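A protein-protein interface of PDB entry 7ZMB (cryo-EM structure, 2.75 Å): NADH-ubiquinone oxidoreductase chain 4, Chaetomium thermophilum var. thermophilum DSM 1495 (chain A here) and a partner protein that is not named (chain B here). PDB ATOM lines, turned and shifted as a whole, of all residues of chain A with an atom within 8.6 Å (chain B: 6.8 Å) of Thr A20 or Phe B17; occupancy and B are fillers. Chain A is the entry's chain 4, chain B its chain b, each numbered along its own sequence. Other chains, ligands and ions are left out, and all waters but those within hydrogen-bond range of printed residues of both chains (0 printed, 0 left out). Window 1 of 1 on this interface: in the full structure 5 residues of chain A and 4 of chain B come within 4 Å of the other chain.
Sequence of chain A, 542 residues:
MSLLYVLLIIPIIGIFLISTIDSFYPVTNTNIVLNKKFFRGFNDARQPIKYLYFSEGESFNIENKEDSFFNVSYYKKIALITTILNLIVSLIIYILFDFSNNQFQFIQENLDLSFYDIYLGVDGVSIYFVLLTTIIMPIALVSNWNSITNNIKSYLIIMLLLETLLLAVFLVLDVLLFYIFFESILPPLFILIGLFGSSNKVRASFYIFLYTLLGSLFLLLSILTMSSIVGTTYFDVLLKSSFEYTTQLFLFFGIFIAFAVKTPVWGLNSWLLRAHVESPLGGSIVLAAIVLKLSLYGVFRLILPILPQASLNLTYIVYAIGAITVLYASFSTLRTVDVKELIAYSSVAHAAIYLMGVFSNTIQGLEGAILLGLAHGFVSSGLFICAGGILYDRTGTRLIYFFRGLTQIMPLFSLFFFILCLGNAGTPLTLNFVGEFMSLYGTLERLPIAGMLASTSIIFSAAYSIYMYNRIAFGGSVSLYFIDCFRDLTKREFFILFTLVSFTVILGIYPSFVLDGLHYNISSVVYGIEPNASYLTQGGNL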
ATOM      1  N   ILE A  13      19.939  -1.733  11.710  1.00  0.00           N
ATOM      2  CA  ILE A  13      19.723  -0.352  12.140  1.00  0.00           C
ATOM      3  C   ILE A  13      18.435   0.187  11.547  1.00  0.00           C
ATOM      4  O   ILE A  13      17.632   0.817  12.244  1.00  0.00           O
ATOM      5  CB  ILE A  13      20.923   0.552  11.791  1.00  0.00           C
ATOM      6  CG1 ILE A  13      22.173   0.163  12.577  1.00  0.00           C
ATOM      7  CG2 ILE A  13      20.589   2.006  12.036  1.00  0.00           C
ATOM      8  CD1 ILE A  13      23.045  -0.818  11.925  1.00  0.00           C
ATOM      9  N   GLY A  14      18.205  -0.074  10.262  1.00  0.00           N
ATOM     10  CA  GLY A  14      16.986   0.397   9.627  1.00  0.00           C
ATOM     11  C   GLY A  14      15.735  -0.124  10.299  1.00  0.00           C
ATOM     12  O   GLY A  14      14.781   0.625  10.512  1.00  0.00           O
ATOM     13  N   ILE A  15      15.724  -1.411  10.653  1.00  0.00           N
ATOM     14  CA  ILE A  15      14.594  -1.976  11.384  1.00  0.00           C
ATOM     15  C   ILE A  15      14.438  -1.281  12.732  1.00  0.00           C
ATOM     16  O   ILE A  15      13.337  -0.872  13.115  1.00  0.00           O
ATOM     17  CB  ILE A  15      14.760  -3.500  11.546  1.00  0.00           C
ATOM     18  CG1 ILE A  15      14.753  -4.188  10.176  1.00  0.00           C
ATOM     19  CG2 ILE A  15      13.664  -4.081  12.450  1.00  0.00           C
ATOM     20  CD1 ILE A  15      15.351  -5.578  10.179  1.00  0.00           C
ATOM     21  N   PHE A  16      15.541  -1.124  13.464  1.00  0.00           N
ATOM     22  CA  PHE A  16      15.477  -0.431  14.748  1.00  0.00           C
ATOM     23  C   PHE A  16      15.101   1.030  14.572  1.00  0.00           C
ATOM     24  O   PHE A  16      14.315   1.574  15.356  1.00  0.00           O
ATOM     25  CB  PHE A  16      16.804  -0.546  15.491  1.00  0.00           C
ATOM     26  CG  PHE A  16      16.788   0.110  16.839  1.00  0.00           C
ATOM     27  CD1 PHE A  16      16.146  -0.497  17.905  1.00  0.00           C
ATOM     28  CD2 PHE A  16      17.407   1.331  17.043  1.00  0.00           C
ATOM     29  CE1 PHE A  16      16.117   0.103  19.149  1.00  0.00           C
ATOM     30  CE2 PHE A  16      17.386   1.934  18.285  1.00  0.00           C
ATOM     31  CZ  PHE A  16      16.741   1.319  19.339  1.00  0.00           C
ATOM     32  N   LEU A  17      15.656   1.690  13.555  1.00  0.00           N
ATOM     33  CA  LEU A  17      15.275   3.074  13.289  1.00  0.00           C
ATOM     34  C   LEU A  17      13.791   3.182  12.983  1.00  0.00           C
ATOM     35  O   LEU A  17      13.097   4.037  13.534  1.00  0.00           O
ATOM     36  CB  LEU A  17      16.097   3.637  12.136  1.00  0.00           C
ATOM     37  CG  LEU A  17      17.543   3.962  12.456  1.00  0.00           C
ATOM     38  CD1 LEU A  17      18.169   4.711  11.301  1.00  0.00           C
ATOM     39  CD2 LEU A  17      17.602   4.775  13.725  1.00  0.00           C
ATOM     40  N   ILE A  18      13.282   2.299  12.125  1.00  0.00           N
ATOM     41  CA  ILE A  18      11.888   2.383  11.700  1.00  0.00           C
ATOM     42  C   ILE A  18      10.945   2.189  12.882  1.00  0.00           C
ATOM     43  O   ILE A  18       9.904   2.848  12.976  1.00  0.00           O
ATOM     44  CB  ILE A  18      11.616   1.363  10.578  1.00  0.00           C
ATOM     45  CG1 ILE A  18      12.139   1.891   9.243  1.00  0.00           C
ATOM     46  CG2 ILE A  18      10.138   1.055  10.477  1.00  0.00           C
ATOM     47  CD1 ILE A  18      12.452   0.814   8.223  1.00  0.00           C
ATOM     48  N   SER A  19      11.289   1.300  13.809  1.00  0.00           N
ATOM     49  CA  SER A  19      10.321   0.917  14.825  1.00  0.00           C
ATOM     50  C   SER A  19      10.257   1.880  16.007  1.00  0.00           C
ATOM     51  O   SER A  19       9.278   1.838  16.761  1.00  0.00           O
ATOM     52  CB  SER A  19      10.605  -0.500  15.325  1.00  0.00           C
ATOM     53  OG  SER A  19      11.973  -0.692  15.626  1.00  0.00           O
ATOM     54  N   THR A  20      11.249   2.750  16.183  1.00  0.00           N
ATOM     55  CA  THR A  20      11.288   3.634  17.341  1.00  0.00           C
ATOM     56  C   THR A  20      10.909   5.077  17.044  1.00  0.00           C
ATOM     57  O   THR A  20      10.745   5.850  17.990  1.00  0.00           O
ATOM     58  CB  THR A  20      12.681   3.637  17.974  1.00  0.00           C
ATOM     59  OG1 THR A  20      13.599   4.287  17.088  1.00  0.00           O
ATOM     60  CG2 THR A  20      13.142   2.231  18.253  1.00  0.00           C
ATOM     61  N   ILE A  21      10.783   5.472  15.778  1.00  0.00           N
ATOM     62  CA  ILE A  21      10.486   6.873  15.479  1.00  0.00           C
ATOM     63  C   ILE A  21       9.133   7.272  16.049  1.00  0.00           C
ATOM     64  O   ILE A  21       8.966   8.385  16.559  1.00  0.00           O
ATOM     65  CB  ILE A  21      10.565   7.140  13.966  1.00  0.00           C
ATOM     66  CG1 ILE A  21      11.956   6.806  13.452  1.00  0.00           C
ATOM     67  CG2 ILE A  21      10.211   8.585  13.648  1.00  0.00           C
ATOM     68  CD1 ILE A  21      13.035   7.634  14.090  1.00  0.00           C
ATOM     69  N   ASP A  22       8.153   6.369  15.993  1.00  0.00           N
ATOM     70  CA  ASP A  22       6.839   6.661  16.555  1.00  0.00           C
ATOM     71  C   ASP A  22       6.920   7.034  18.028  1.00  0.00           C
ATOM     72  O   ASP A  22       6.036   7.737  18.530  1.00  0.00           O
ATOM     73  CB  ASP A  22       5.905   5.463  16.369  1.00  0.00           C
ATOM     74  CG  ASP A  22       4.466   5.782  16.737  1.00  0.00           C
ATOM     75  OD1 ASP A  22       3.756   6.382  15.905  1.00  0.00           O
ATOM     76  OD2 ASP A  22       4.047   5.432  17.861  1.00  0.00           O
ATOM     77  N   SER A  23       7.961   6.587  18.724  1.00  0.00           N
ATOM     78  CA  SER A  23       8.221   6.992  20.097  1.00  0.00           C
ATOM     79  C   SER A  23       8.927   8.338  20.192  1.00  0.00           C
ATOM     80  O   SER A  23       9.103   8.849  21.302  1.00  0.00           O
ATOM     81  CB  SER A  23       9.067   5.929  20.800  1.00  0.00           C
ATOM     82  OG  SER A  23      10.368   5.888  20.243  1.00  0.00           O
ATOM     83  N   PHE A  24       9.332   8.918  19.064  1.00  0.00           N
ATOM     84  CA  PHE A  24      10.127  10.139  19.048  1.00  0.00           C
ATOM     85  C   PHE A  24       9.358  11.338  18.520  1.00  0.00           C
ATOM     86  O   PHE A  24       9.243  12.352  19.217  1.00  0.00           O
ATOM     87  CB  PHE A  24      11.383   9.925  18.195  1.00  0.00           C
ATOM     88  CG  PHE A  24      12.375   8.990  18.803  1.00  0.00           C
ATOM     89  CD1 PHE A  24      12.638   9.023  20.160  1.00  0.00           C
ATOM     90  CD2 PHE A  24      13.041   8.064  18.019  1.00  0.00           C
ATOM     91  CE1 PHE A  24      13.555   8.158  20.720  1.00  0.00           C
ATOM     92  CE2 PHE A  24      13.954   7.197  18.575  1.00  0.00           C
ATOM     93  CZ  PHE A  24      14.211   7.245  19.925  1.00  0.00           C
ATOM     94  N   TYR A  25       8.829  11.251  17.304  1.00  0.00           N
ATOM     95  CA  TYR A  25       8.172  12.385  16.664  1.00  0.00           C
ATOM     96  C   TYR A  25       6.727  12.525  17.131  1.00  0.00           C
ATOM     97  O   TYR A  25       6.445  12.497  18.329  1.00  0.00           O
ATOM     98  CB  TYR A  25       8.223  12.236  15.140  1.00  0.00           C
ATOM     99  CG  TYR A  25       9.473  12.802  14.505  1.00  0.00           C
ATOM    100  CD1 TYR A  25      10.723  12.573  15.063  1.00  0.00           C
ATOM    101  CD2 TYR A  25       9.405  13.554  13.339  1.00  0.00           C
ATOM    102  CE1 TYR A  25      11.871  13.084  14.483  1.00  0.00           C
ATOM    103  CE2 TYR A  25      10.547  14.069  12.753  1.00  0.00           C
ATOM    104  CZ  TYR A  25      11.776  13.831  13.329  1.00  0.00           C
ATOM    105  OH  TYR A  25      12.916  14.340  12.750  1.00  0.00           O
ATOM    106  N   PHE A  70       3.509   9.810  13.258  1.00  0.00           N
ATOM    107  CA  PHE A  70       4.523  10.008  12.232  1.00  0.00           C
ATOM    108  C   PHE A  70       4.011   9.537  10.877  1.00  0.00           C
ATOM    109  O   PHE A  70       3.323   8.518  10.772  1.00  0.00           O
ATOM    110  CB  PHE A  70       5.804   9.262  12.598  1.00  0.00           C
ATOM    111  N   TYR A  75       9.065   6.353   7.015  1.00  0.00           N
ATOM    112  CA  TYR A  75       9.635   5.028   7.208  1.00  0.00           C
ATOM    113  C   TYR A  75      10.128   4.434   5.896  1.00  0.00           C
ATOM    114  O   TYR A  75      11.106   3.681   5.889  1.00  0.00           O
ATOM    115  CB  TYR A  75       8.610   4.130   7.901  1.00  0.00           C
ATOM    116  CG  TYR A  75       8.179   4.719   9.218  1.00  0.00           C
ATOM    117  CD1 TYR A  75       8.927   4.514  10.359  1.00  0.00           C
ATOM    118  CD2 TYR A  75       7.041   5.506   9.312  1.00  0.00           C
ATOM    119  CE1 TYR A  75       8.564   5.067  11.555  1.00  0.00           C
ATOM    120  CE2 TYR A  75       6.658   6.065  10.519  1.00  0.00           C
ATOM    121  CZ  TYR A  75       7.429   5.840  11.638  1.00  0.00           C
ATOM    122  OH  TYR A  75       7.067   6.376  12.852  1.00  0.00           O
ATOM    123  N   ILE A  78      13.561   6.001   5.376  1.00  0.00           N
ATOM    124  CA  ILE A  78      14.600   5.293   6.117  1.00  0.00           C
ATOM    125  C   ILE A  78      14.931   3.970   5.444  1.00  0.00           C
ATOM    126  O   ILE A  78      16.100   3.609   5.287  1.00  0.00           O
ATOM    127  CB  ILE A  78      14.170   5.076   7.580  1.00  0.00           C
ATOM    128  CG1 ILE A  78      13.776   6.391   8.242  1.00  0.00           C
ATOM    129  CG2 ILE A  78      15.256   4.355   8.362  1.00  0.00           C
ATOM    130  CD1 ILE A  78      13.493   6.236   9.715  1.00  0.00           C
ATOM    131  N   LYS A 153       5.016  -0.388   8.015  1.00  0.00           N
ATOM    132  CA  LYS A 153       6.118  -0.753   8.896  1.00  0.00           C
ATOM    133  C   LYS A 153       6.468  -2.222   8.745  1.00  0.00           C
ATOM    134  O   LYS A 153       7.645  -2.580   8.665  1.00  0.00           O
ATOM    135  CB  LYS A 153       5.760  -0.471  10.349  1.00  0.00           C
ATOM    136  CG  LYS A 153       5.598   0.957  10.700  1.00  0.00           C
ATOM    137  CD  LYS A 153       5.301   1.077  12.167  1.00  0.00           C
ATOM    138  CE  LYS A 153       5.039   2.512  12.523  1.00  0.00           C
ATOM    139  NZ  LYS A 153       6.256   3.298  12.371  1.00  0.00           N
ATOM    140  N   ILE A 157       9.976  -3.671   7.387  1.00  0.00           N
ATOM    141  CA  ILE A 157      10.811  -4.421   8.322  1.00  0.00           C
ATOM    142  C   ILE A 157      11.131  -5.800   7.765  1.00  0.00           C
ATOM    143  O   ILE A 157      12.264  -6.278   7.883  1.00  0.00           O
ATOM    144  CB  ILE A 157      10.141  -4.503   9.703  1.00  0.00           C
ATOM    145  CG1 ILE A 157      10.449  -3.250  10.516  1.00  0.00           C
ATOM    146  CG2 ILE A 157      10.616  -5.714  10.467  1.00  0.00           C
ATOM    147  CD1 ILE A 157       9.510  -3.032  11.660  1.00  0.00           C
ATOM    148  N   GLY B  12      19.771  -7.547  27.609  1.00  0.00           N
ATOM    149  CA  GLY B  12      18.890  -6.971  28.608  1.00  0.00           C
ATOM    150  C   GLY B  12      18.131  -5.768  28.095  1.00  0.00           C
ATOM    151  O   GLY B  12      16.976  -5.554  28.463  1.00  0.00           O
ATOM    152  N   LEU B  13      18.764  -4.977  27.229  1.00  0.00           N
ATOM    153  CA  LEU B  13      18.088  -3.841  26.620  1.00  0.00           C
ATOM    154  C   LEU B  13      16.924  -4.289  25.748  1.00  0.00           C
ATOM    155  O   LEU B  13      15.869  -3.646  25.736  1.00  0.00           O
ATOM    156  CB  LEU B  13      19.082  -3.023  25.800  1.00  0.00           C
ATOM    157  CG  LEU B  13      20.182  -2.305  26.576  1.00  0.00           C
ATOM    158  CD1 LEU B  13      21.136  -1.657  25.611  1.00  0.00           C
ATOM    159  CD2 LEU B  13      19.594  -1.282  27.499  1.00  0.00           C
ATOM    160  N   ALA B  14      17.099  -5.381  25.003  1.00  0.00           N
ATOM    161  CA  ALA B  14      16.042  -5.869  24.128  1.00  0.00           C
ATOM    162  C   ALA B  14      14.893  -6.514  24.890  1.00  0.00           C
ATOM    163  O   ALA B  14      13.769  -6.528  24.381  1.00  0.00           O
ATOM    164  CB  ALA B  14      16.610  -6.857  23.112  1.00  0.00           C
ATOM    165  N   VAL B  15      15.139  -7.059  26.079  1.00  0.00           N
ATOM    166  CA  VAL B  15      14.030  -7.543  26.893  1.00  0.00           C
ATOM    167  C   VAL B  15      13.117  -6.387  27.279  1.00  0.00           C
ATOM    168  O   VAL B  15      11.890  -6.487  27.187  1.00  0.00           O
ATOM    169  CB  VAL B  15      14.549  -8.292  28.131  1.00  0.00           C
ATOM    170  CG1 VAL B  15      13.392  -8.677  29.033  1.00  0.00           C
ATOM    171  CG2 VAL B  15      15.347  -9.513  27.727  1.00  0.00           C
ATOM    172  N   ARG B  16      13.703  -5.269  27.702  1.00  0.00           N
ATOM    173  CA  ARG B  16      12.912  -4.094  28.045  1.00  0.00           C
ATOM    174  C   ARG B  16      12.163  -3.564  26.830  1.00  0.00           C
ATOM    175  O   ARG B  16      11.012  -3.134  26.941  1.00  0.00           O
ATOM    176  CB  ARG B  16      13.824  -3.028  28.644  1.00  0.00           C
ATOM    177  CG  ARG B  16      13.132  -1.809  29.209  1.00  0.00           C
ATOM    178  CD  ARG B  16      12.112  -2.120  30.271  1.00  0.00           C
ATOM    179  NE  ARG B  16      11.323  -0.932  30.559  1.00  0.00           N
ATOM    180  CZ  ARG B  16      10.400  -0.841  31.507  1.00  0.00           C
ATOM    181  NH1 ARG B  16       9.746   0.295  31.682  1.00  0.00           N
ATOM    182  NH2 ARG B  16      10.129  -1.878  32.272  1.00  0.00           N
ATOM    183  N   PHE B  17      12.801  -3.592  25.659  1.00  0.00           N
ATOM    184  CA  PHE B  17      12.120  -3.200  24.430  1.00  0.00           C
ATOM    185  C   PHE B  17      10.958  -4.130  24.127  1.00  0.00           C
ATOM    186  O   PHE B  17       9.840  -3.684  23.853  1.00  0.00           O
ATOM    187  CB  PHE B  17      13.107  -3.203  23.269  1.00  0.00           C
ATOM    188  CG  PHE B  17      12.764  -2.236  22.189  1.00  0.00           C
ATOM    189  CD1 PHE B  17      12.612  -0.888  22.476  1.00  0.00           C
ATOM    190  CD2 PHE B  17      12.570  -2.668  20.893  1.00  0.00           C
ATOM    191  CE1 PHE B  17      12.294   0.010  21.485  1.00  0.00           C
ATOM    192  CE2 PHE B  17      12.250  -1.775  19.900  1.00  0.00           C
ATOM    193  CZ  PHE B  17      12.108  -0.433  20.197  1.00  0.00           C
ATOM    194  N   TRP B  18      11.204  -5.441  24.176  1.00  0.00           N
ATOM    195  CA  TRP B  18      10.152  -6.394  23.856  1.00  0.00           C
ATOM    196  C   TRP B  18       9.054  -6.369  24.904  1.00  0.00           C
ATOM    197  O   TRP B  18       7.879  -6.571  24.582  1.00  0.00           O
ATOM    198  CB  TRP B  18      10.743  -7.791  23.714  1.00  0.00           C
ATOM    199  CG  TRP B  18      11.168  -8.115  22.326  1.00  0.00           C
ATOM    200  CD1 TRP B  18      12.312  -7.709  21.706  1.00  0.00           C
ATOM    201  CD2 TRP B  18      10.461  -8.915  21.378  1.00  0.00           C
ATOM    202  NE1 TRP B  18      12.358  -8.203  20.427  1.00  0.00           N
ATOM    203  CE2 TRP B  18      11.235  -8.951  20.203  1.00  0.00           C
ATOM    204  CE3 TRP B  18       9.251  -9.606  21.406  1.00  0.00           C
ATOM    205  CZ2 TRP B  18      10.833  -9.647  19.069  1.00  0.00           C
ATOM    206  CZ3 TRP B  18       8.858 -10.289  20.280  1.00  0.00           C
ATOM    207  CH2 TRP B  18       9.645 -10.310  19.131  1.00  0.00           C
ATOM    208  N   GLN B  19       9.416  -6.112  26.162  1.00  0.00           N
ATOM    209  CA  GLN B  19       8.412  -5.959  27.208  1.00  0.00           C
ATOM    210  C   GLN B  19       7.421  -4.865  26.865  1.00  0.00           C
ATOM    211  O   GLN B  19       6.204  -5.070  26.912  1.00  0.00           O
ATOM    212  CB  GLN B  19       9.067  -5.603  28.531  1.00  0.00           C
ATOM    213  CG  GLN B  19       8.049  -5.472  29.627  1.00  0.00           C
ATOM    214  CD  GLN B  19       8.660  -5.084  30.925  1.00  0.00           C
ATOM    215  OE1 GLN B  19       9.860  -4.865  31.012  1.00  0.00           O
ATOM    216  NE2 GLN B  19       7.836  -4.975  31.954  1.00  0.00           N
ATOM    217  N   LEU B  20       7.935  -3.677  26.552  1.00  0.00           N
ATOM    218  CA  LEU B  20       7.071  -2.530  26.322  1.00  0.00           C
ATOM    219  C   LEU B  20       6.245  -2.721  25.060  1.00  0.00           C
ATOM    220  O   LEU B  20       5.088  -2.290  24.998  1.00  0.00           O
ATOM    221  CB  LEU B  20       7.917  -1.262  26.249  1.00  0.00           C
ATOM    222  CG  LEU B  20       8.715  -0.963  27.523  1.00  0.00           C
ATOM    223  CD1 LEU B  20       9.657   0.213  27.345  1.00  0.00           C
ATOM    224  CD2 LEU B  20       7.787  -0.741  28.700  1.00  0.00           C
ATOM    225  N   GLY B  21       6.822  -3.404  24.078  1.00  0.00           N
ATOM    226  CA  GLY B  21       6.068  -3.705  22.853  1.00  0.00           C
ATOM    227  C   GLY B  21       4.929  -4.650  23.152  1.00  0.00           C
ATOM    228  O   GLY B  21       3.802  -4.359  22.717  1.00  0.00           O
ATOM    229  N   ILE B  22       5.205  -5.755  23.852  1.00  0.00           N
ATOM    230  CA  ILE B  22       4.112  -6.695  24.247  1.00  0.00           C
ATOM    231  C   ILE B  22       3.090  -5.944  25.105  1.00  0.00           C
ATOM    232  O   ILE B  22       1.894  -6.111  24.863  1.00  0.00           O
ATOM    233  CB  ILE B  22       4.679  -7.932  24.973  1.00  0.00           C
ATOM    234  CG1 ILE B  22       5.281  -8.937  23.989  1.00  0.00           C
ATOM    235  CG2 ILE B  22       3.644  -8.582  25.877  1.00  0.00           C
ATOM    236  CD1 ILE B  22       6.179  -9.953  24.640  1.00  0.00           C
ATOM    237  N   ARG B  25       3.241  -0.366  25.633  1.00  0.00           N
ATOM    238  CA  ARG B  25       3.549   0.890  26.360  1.00  0.00           C
ATOM    239  C   ARG B  25       4.610   1.669  25.566  1.00  0.00           C
ATOM    240  O   ARG B  25       5.461   1.011  24.949  1.00  0.00           O
ATOM    241  CB  ARG B  25       4.029   0.601  27.785  1.00  0.00           C
ATOM    242  CG  ARG B  25       2.928   0.292  28.785  1.00  0.00           C
ATOM    243  CD  ARG B  25       3.585  -0.049  30.103  1.00  0.00           C
ATOM    244  NE  ARG B  25       4.783   0.755  30.267  1.00  0.00           N
ATOM    245  CZ  ARG B  25       5.672   0.590  31.235  1.00  0.00           C
ATOM    246  NH1 ARG B  25       6.734   1.374  31.297  1.00  0.00           N
ATOM    247  NH2 ARG B  25       5.501  -0.360  32.135  1.00  0.00           N
ATOM    248  N   PHE B  27       7.844   3.144  24.086  1.00  0.00           N
ATOM    249  CA  PHE B  27       9.275   3.057  24.316  1.00  0.00           C
ATOM    250  C   PHE B  27       9.806   4.443  24.653  1.00  0.00           C
ATOM    251  O   PHE B  27       9.293   5.460  24.179  1.00  0.00           O
ATOM    252  CB  PHE B  27      10.006   2.536  23.080  1.00  0.00           C
ATOM    253  CG  PHE B  27       9.423   1.293  22.489  1.00  0.00           C
ATOM    254  CD1 PHE B  27       9.476   0.093  23.160  1.00  0.00           C
ATOM    255  CD2 PHE B  27       8.873   1.318  21.225  1.00  0.00           C
ATOM    256  CE1 PHE B  27       8.955  -1.053  22.594  1.00  0.00           C
ATOM    257  CE2 PHE B  27       8.352   0.182  20.658  1.00  0.00           C
ATOM    258  CZ  PHE B  27       8.399  -1.008  21.342  1.00  0.00           C
ATOM    259  N   PHE B  28      10.834   4.481  25.491  1.00  0.00           N
ATOM    260  CA  PHE B  28      11.599   5.699  25.744  1.00  0.00           C
ATOM    261  C   PHE B  28      10.766   6.786  26.410  1.00  0.00           C
ATOM    262  O   PHE B  28      11.018   7.976  26.224  1.00  0.00           O
ATOM    263  CB  PHE B  28      12.234   6.215  24.454  1.00  0.00           C
ATOM    264  CG  PHE B  28      13.070   5.192  23.751  1.00  0.00           C
ATOM    265  CD1 PHE B  28      13.781   4.251  24.468  1.00  0.00           C
ATOM    266  CD2 PHE B  28      13.152   5.174  22.378  1.00  0.00           C
ATOM    267  CE1 PHE B  28      14.552   3.312  23.826  1.00  0.00           C
ATOM    268  CE2 PHE B  28      13.928   4.242  21.736  1.00  0.00           C
ATOM    269  CZ  PHE B  28      14.628   3.311  22.463  1.00  0.00           C
ATOM    270  N   TYR B  36      16.371   0.884  31.363  1.00  0.00           N
ATOM    271  CA  TYR B  36      17.281   0.396  30.344  1.00  0.00           C
ATOM    272  C   TYR B  36      18.671   0.177  30.933  1.00  0.00           C
ATOM    273  O   TYR B  36      19.302  -0.844  30.640  1.00  0.00           O
ATOM    274  CB  TYR B  36      17.299   1.350  29.150  1.00  0.00           C
ATOM    275  CG  TYR B  36      16.078   1.194  28.275  1.00  0.00           C
ATOM    276  CD1 TYR B  36      15.997   0.166  27.357  1.00  0.00           C
ATOM    277  CD2 TYR B  36      15.002   2.058  28.387  1.00  0.00           C
ATOM    278  CE1 TYR B  36      14.888   0.004  26.564  1.00  0.00           C
ATOM    279  CE2 TYR B  36      13.883   1.903  27.594  1.00  0.00           C
ATOM    280  CZ  TYR B  36      13.834   0.870  26.681  1.00  0.00           C
ATOM    281  OH  TYR B  36      12.736   0.691  25.880  1.00  0.00           O
ATOM    282  N   PHE B  39      17.677  -3.158  33.294  1.00  0.00           N
ATOM    283  CA  PHE B  39      17.651  -4.363  32.476  1.00  0.00           C
ATOM    284  C   PHE B  39      19.000  -4.597  31.813  1.00  0.00           C
ATOM    285  O   PHE B  39      19.466  -5.738  31.738  1.00  0.00           O
ATOM    286  CB  PHE B  39      16.559  -4.251  31.415  1.00  0.00           C
ATOM    287  CG  PHE B  39      15.159  -4.446  31.933  1.00  0.00           C
ATOM    288  CD1 PHE B  39      14.667  -3.679  32.980  1.00  0.00           C
ATOM    289  CD2 PHE B  39      14.334  -5.394  31.369  1.00  0.00           C
ATOM    290  CE1 PHE B  39      13.383  -3.851  33.439  1.00  0.00           C
ATOM    291  CE2 PHE B  39      13.048  -5.558  31.819  1.00  0.00           C
ATOM    292  CZ  PHE B  39      12.573  -4.788  32.862  1.00  0.00           C
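The backbone carbonyl oxygen (O) of Phe A16 sits close to the side-chain hydroxyl (OG1) of Thr A20 (3.3 Å).
Among the printed residues, pairs that only touch across the chains: Thr A20 with Phe B17, Ser A23 with Phe B27, Ser A23 with Phe B28 and Phe A24 with Phe B28.
Printed residues of chain B within 4 Å of Thr A20: Phe B17 (3.5 Å). Printed residues of chain B within 4 Å of Ser A23: Phe B27 and Phe B28. Printed residues of chain B within 4 Å of Phe A24: Phe B28. Tyr A25 touches none of the printed residues of chain B. Phe B17 touches one residue of chain A. Of the printed residues of chain A, Phe B27 touches Ser A23 (3.4 Å). Of the printed residues of chain A, Phe B28 touches Ser A23 and Phe A24.
Along chain B the printed residues that touch a printed residue of chain A span positions 17 to 28. Of the 18 printed residues of chain A, 3 touch a printed residue of chain B. Printed residues of chain A that touch a printed residue of chain B: Thr A20, Ser A23 and Phe A24.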
